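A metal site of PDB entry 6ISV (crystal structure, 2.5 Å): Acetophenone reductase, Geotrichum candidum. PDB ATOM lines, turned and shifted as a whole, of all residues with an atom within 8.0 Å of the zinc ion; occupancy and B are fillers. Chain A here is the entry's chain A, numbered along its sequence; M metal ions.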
ATOM      1  N   ASN A  96       4.402  -1.563  -1.886  1.00  0.00           N
ATOM      2  CA  ASN A  96       5.722  -2.179  -1.976  1.00  0.00           C
ATOM      3  C   ASN A  96       6.250  -2.581  -0.601  1.00  0.00           C
ATOM      4  O   ASN A  96       7.324  -2.116  -0.200  1.00  0.00           O
ATOM      5  CB  ASN A  96       6.658  -1.205  -2.710  1.00  0.00           C
ATOM      6  CG  ASN A  96       7.998  -1.808  -3.071  1.00  0.00           C
ATOM      7  OD1 ASN A  96       8.141  -3.040  -3.202  1.00  0.00           O
ATOM      8  ND2 ASN A  96       9.003  -0.951  -3.256  1.00  0.00           N
ATOM      9  N   PRO A  97       5.540  -3.412   0.163  1.00  0.00           N
ATOM     10  CA  PRO A  97       6.002  -3.767   1.513  1.00  0.00           C
ATOM     11  C   PRO A  97       7.284  -4.587   1.477  1.00  0.00           C
ATOM     12  O   PRO A  97       7.646  -5.208   0.479  1.00  0.00           O
ATOM     13  CB  PRO A  97       4.834  -4.594   2.068  1.00  0.00           C
ATOM     14  CG  PRO A  97       4.287  -5.255   0.866  1.00  0.00           C
ATOM     15  CD  PRO A  97       4.389  -4.241  -0.253  1.00  0.00           C
ATOM     16  N   CYS A  98       7.972  -4.597   2.627  1.00  0.00           N
ATOM     17  CA  CYS A  98       9.199  -5.376   2.682  1.00  0.00           C
ATOM     18  C   CYS A  98       8.906  -6.876   2.764  1.00  0.00           C
ATOM     19  O   CYS A  98       9.670  -7.683   2.234  1.00  0.00           O
ATOM     20  CB  CYS A  98      10.058  -4.919   3.863  1.00  0.00           C
ATOM     21  SG  CYS A  98       9.522  -5.481   5.485  1.00  0.00           S
ATOM     22  N   GLY A  99       7.790  -7.258   3.372  1.00  0.00           N
ATOM     23  CA  GLY A  99       7.338  -8.632   3.414  1.00  0.00           C
ATOM     24  C   GLY A  99       7.703  -9.349   4.696  1.00  0.00           C
ATOM     25  O   GLY A  99       7.165 -10.438   4.952  1.00  0.00           O
ATOM     26  N   SER A 100       8.549  -8.747   5.520  1.00  0.00           N
ATOM     27  CA  SER A 100       9.147  -9.427   6.665  1.00  0.00           C
ATOM     28  C   SER A 100       9.062  -8.664   7.977  1.00  0.00           C
ATOM     29  O   SER A 100       9.431  -9.219   9.017  1.00  0.00           O
ATOM     30  CB  SER A 100      10.623  -9.712   6.385  1.00  0.00           C
ATOM     31  OG  SER A 100      11.351  -9.730   7.595  1.00  0.00           O
ATOM     32  N   CYS A 101       8.622  -7.399   7.977  1.00  0.00           N
ATOM     33  CA  CYS A 101       8.664  -6.623   9.213  1.00  0.00           C
ATOM     34  C   CYS A 101       7.439  -6.923  10.061  1.00  0.00           C
ATOM     35  O   CYS A 101       6.592  -7.759   9.707  1.00  0.00           O
ATOM     36  CB  CYS A 101       8.760  -5.135   8.893  1.00  0.00           C
ATOM     37  SG  CYS A 101       7.183  -4.523   8.233  1.00  0.00           S
ATOM     38  N   ARG A 102       7.308  -6.219  11.198  1.00  0.00           N
ATOM     39  CA  ARG A 102       6.166  -6.455  12.080  1.00  0.00           C
ATOM     40  C   ARG A 102       4.849  -6.105  11.392  1.00  0.00           C
ATOM     41  O   ARG A 102       3.842  -6.809  11.557  1.00  0.00           O
ATOM     42  CB  ARG A 102       6.310  -5.632  13.364  1.00  0.00           C
ATOM     43  CG  ARG A 102       7.502  -5.949  14.236  1.00  0.00           C
ATOM     44  CD  ARG A 102       7.154  -6.970  15.302  1.00  0.00           C
ATOM     45  NE  ARG A 102       8.365  -7.389  16.002  1.00  0.00           N
ATOM     46  CZ  ARG A 102       8.637  -7.109  17.268  1.00  0.00           C
ATOM     47  NH1 ARG A 102       7.767  -6.426  17.997  1.00  0.00           N
ATOM     48  NH2 ARG A 102       9.778  -7.524  17.813  1.00  0.00           N
ATOM     49  N   GLU A 103       4.842  -5.009  10.628  1.00  0.00           N
ATOM     50  CA  GLU A 103       3.622  -4.596   9.945  1.00  0.00           C
ATOM     51  C   GLU A 103       3.248  -5.554   8.814  1.00  0.00           C
ATOM     52  O   GLU A 103       2.072  -5.852   8.603  1.00  0.00           O
ATOM     53  CB  GLU A 103       3.779  -3.162   9.441  1.00  0.00           C
ATOM     54  CG  GLU A 103       3.178  -2.128  10.378  1.00  0.00           C
ATOM     55  CD  GLU A 103       4.139  -1.605  11.442  1.00  0.00           C
ATOM     56  OE1 GLU A 103       5.340  -1.963  11.418  1.00  0.00           O
ATOM     57  OE2 GLU A 103       3.677  -0.836  12.320  1.00  0.00           O
ATOM     58  N   CYS A 104       4.244  -6.092   8.107  1.00  0.00           N
ATOM     59  CA  CYS A 104       3.955  -7.007   7.015  1.00  0.00           C
ATOM     60  C   CYS A 104       3.424  -8.336   7.549  1.00  0.00           C
ATOM     61  O   CYS A 104       2.446  -8.874   7.018  1.00  0.00           O
ATOM     62  CB  CYS A 104       5.212  -7.177   6.165  1.00  0.00           C
ATOM     63  SG  CYS A 104       5.681  -5.613   5.396  1.00  0.00           S
ATOM     64  N   ARG A 105       4.003  -8.843   8.650  1.00  0.00           N
ATOM     65  CA  ARG A 105       3.540 -10.121   9.208  1.00  0.00           C
ATOM     66  C   ARG A 105       2.207  -9.975   9.925  1.00  0.00           C
ATOM     67  O   ARG A 105       1.440 -10.949  10.016  1.00  0.00           O
ATOM     68  CB  ARG A 105       4.577 -10.686  10.160  1.00  0.00           C
ATOM     69  CG  ARG A 105       5.880 -11.055   9.494  1.00  0.00           C
ATOM     70  CD  ARG A 105       6.984 -11.351  10.505  1.00  0.00           C
ATOM     71  NE  ARG A 105       8.234 -11.602   9.797  1.00  0.00           N
ATOM     72  CZ  ARG A 105       8.544 -12.731   9.158  1.00  0.00           C
ATOM     73  NH1 ARG A 105       7.685 -13.753   9.159  1.00  0.00           N
ATOM     74  NH2 ARG A 105       9.703 -12.835   8.537  1.00  0.00           N
ATOM     75  N   LYS A 108      -1.027  -6.068   8.025  1.00  0.00           N
ATOM     76  CA  LYS A 108      -1.129  -4.652   7.744  1.00  0.00           C
ATOM     77  C   LYS A 108       0.076  -4.193   6.927  1.00  0.00           C
ATOM     78  O   LYS A 108       0.764  -3.245   7.316  1.00  0.00           O
ATOM     79  CB  LYS A 108      -1.208  -3.853   9.048  1.00  0.00           C
ATOM     80  CG  LYS A 108      -2.459  -4.071   9.865  1.00  0.00           C
ATOM     81  CD  LYS A 108      -2.290  -3.425  11.228  1.00  0.00           C
ATOM     82  CE  LYS A 108      -3.389  -3.882  12.172  1.00  0.00           C
ATOM     83  NZ  LYS A 108      -3.151  -3.401  13.568  1.00  0.00           N
ATOM     84  N   ASP A 109       0.342  -4.866   5.802  1.00  0.00           N
ATOM     85  CA  ASP A 109       1.555  -4.515   5.067  1.00  0.00           C
ATOM     86  C   ASP A 109       1.378  -3.304   4.175  1.00  0.00           C
ATOM     87  O   ASP A 109       2.360  -2.816   3.623  1.00  0.00           O
ATOM     88  CB  ASP A 109       2.103  -5.707   4.262  1.00  0.00           C
ATOM     89  CG  ASP A 109       1.179  -6.153   3.135  1.00  0.00           C
ATOM     90  OD1 ASP A 109      -0.028  -6.312   3.343  1.00  0.00           O
ATOM     91  OD2 ASP A 109       1.690  -6.383   2.021  1.00  0.00           O
ATOM     92  N   ASN A 110       0.160  -2.762   4.035  1.00  0.00           N
ATOM     93  CA  ASN A 110       0.020  -1.443   3.445  1.00  0.00           C
ATOM     94  C   ASN A 110       0.691  -0.393   4.314  1.00  0.00           C
ATOM     95  O   ASN A 110       0.967   0.723   3.839  1.00  0.00           O
ATOM     96  CB  ASN A 110      -1.470  -1.103   3.212  1.00  0.00           C
ATOM     97  CG  ASN A 110      -2.262  -0.937   4.524  1.00  0.00           C
ATOM     98  OD1 ASN A 110      -2.250  -1.805   5.398  1.00  0.00           O
ATOM     99  ND2 ASN A 110      -2.981   0.183   4.641  1.00  0.00           N
ATOM    100  N   LEU A 111       0.988  -0.734   5.574  1.00  0.00           N
ATOM    101  CA  LEU A 111       1.570   0.183   6.544  1.00  0.00           C
ATOM    102  C   LEU A 111       3.058  -0.035   6.746  1.00  0.00           C
ATOM    103  O   LEU A 111       3.631   0.507   7.705  1.00  0.00           O
ATOM    104  CB  LEU A 111       0.850   0.056   7.895  1.00  0.00           C
ATOM    105  CG  LEU A 111      -0.662   0.256   7.927  1.00  0.00           C
ATOM    106  CD1 LEU A 111      -1.137   0.142   9.355  1.00  0.00           C
ATOM    107  CD2 LEU A 111      -1.019   1.593   7.372  1.00  0.00           C
ATOM    108  N   CYS A 112       3.710  -0.796   5.875  1.00  0.00           N
ATOM    109  CA  CYS A 112       5.135  -1.066   6.022  1.00  0.00           C
ATOM    110  C   CYS A 112       5.910   0.241   5.939  1.00  0.00           C
ATOM    111  O   CYS A 112       5.697   1.047   5.037  1.00  0.00           O
ATOM    112  CB  CYS A 112       5.606  -2.017   4.919  1.00  0.00           C
ATOM    113  SG  CYS A 112       7.383  -2.424   4.982  1.00  0.00           S
ATOM    114  N   HIS A 113       6.801   0.448   6.906  1.00  0.00           N
ATOM    115  CA  HIS A 113       7.792   1.514   6.897  1.00  0.00           C
ATOM    116  C   HIS A 113       9.165   0.927   7.226  1.00  0.00           C
ATOM    117  O   HIS A 113       9.910   1.451   8.061  1.00  0.00           O
ATOM    118  CB  HIS A 113       7.432   2.633   7.863  1.00  0.00           C
ATOM    119  CG  HIS A 113       7.058   2.168   9.234  1.00  0.00           C
ATOM    120  ND1 HIS A 113       7.985   2.038  10.243  1.00  0.00           N
ATOM    121  CD2 HIS A 113       5.876   1.801   9.760  1.00  0.00           C
ATOM    122  CE1 HIS A 113       7.384   1.610  11.345  1.00  0.00           C
ATOM    123  NE2 HIS A 113       6.099   1.458  11.077  1.00  0.00           N
ATOM    124  N   ALA A 114       9.468  -0.208   6.605  1.00  0.00           N
ATOM    125  CA  ALA A 114      10.795  -0.793   6.710  1.00  0.00           C
ATOM    126  C   ALA A 114      11.792   0.067   5.954  1.00  0.00           C
ATOM    127  O   ALA A 114      11.526   0.481   4.823  1.00  0.00           O
ATOM    128  CB  ALA A 114      10.790  -2.211   6.148  1.00  0.00           C
ATOM    129  N   GLU A 115      12.944   0.317   6.571  1.00  0.00           N
ATOM    130  CA  GLU A 115      13.949   1.208   6.011  1.00  0.00           C
ATOM    131  C   GLU A 115      14.604   0.646   4.750  1.00  0.00           C
ATOM    132  O   GLU A 115      15.548   1.233   4.225  1.00  0.00           O
ATOM    133  CB  GLU A 115      15.020   1.511   7.075  1.00  0.00           C
ATOM    134  N   ASN A 116      14.105  -0.473   4.228  1.00  0.00           N
ATOM    135  CA  ASN A 116      14.693  -1.049   3.036  1.00  0.00           C
ATOM    136  C   ASN A 116      14.136  -0.449   1.758  1.00  0.00           C
ATOM    137  O   ASN A 116      14.852  -0.374   0.752  1.00  0.00           O
ATOM    138  CB  ASN A 116      14.502  -2.572   3.019  1.00  0.00           C
ATOM    139  N   ARG A 117      12.899   0.045   1.789  1.00  0.00           N
ATOM    140  CA  ARG A 117      12.199   0.436   0.575  1.00  0.00           C
ATOM    141  C   ARG A 117      11.236   1.581   0.934  1.00  0.00           C
ATOM    142  O   ARG A 117      11.173   2.006   2.090  1.00  0.00           O
ATOM    143  CB  ARG A 117      11.551  -0.815  -0.020  1.00  0.00           C
ATOM    144  CG  ARG A 117      10.146  -1.078   0.466  1.00  0.00           C
ATOM    145  CD  ARG A 117       9.993  -1.300   1.966  1.00  0.00           C
ATOM    146  NE  ARG A 117       8.616  -0.913   2.275  1.00  0.00           N
ATOM    147  CZ  ARG A 117       8.242   0.284   2.715  1.00  0.00           C
ATOM    148  NH1 ARG A 117       6.961   0.539   2.922  1.00  0.00           N
ATOM    149  NH2 ARG A 117       9.154   1.185   3.005  1.00  0.00           N
HETATM  150 ZN    ZN M   1       7.454  -4.489   6.030  1.00  0.00          ZN
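SG of Cys 104 lies close to N of Gly 99.
The side-chain sulfur (SG) of Cys 101 sits close to the backbone NH (N) of Glu 103 (3.4 Å).
The side-chain sulfur (SG) of Cys 112 sits close to the backbone NH (N) of Ala 114 (3.4 Å).
The backbone carbonyl oxygen (O) of Cys 112 lies within hydrogen-bond range of the guanidinium group (NH1) of Arg 117.
The side-chain sulfur of Cys 98 sits close to the backbone NH of Ser 100 (3.4 Å).
Gly 99 touches the zinc ion (N to ZN, 3.9 Å).
The zinc ion is bound by SG of Cys 104 (2.2 Å), SG of Cys 101 (2.2 Å), SG of Cys 112 (2.3 Å) and SG of Cys 98 (2.4 Å).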
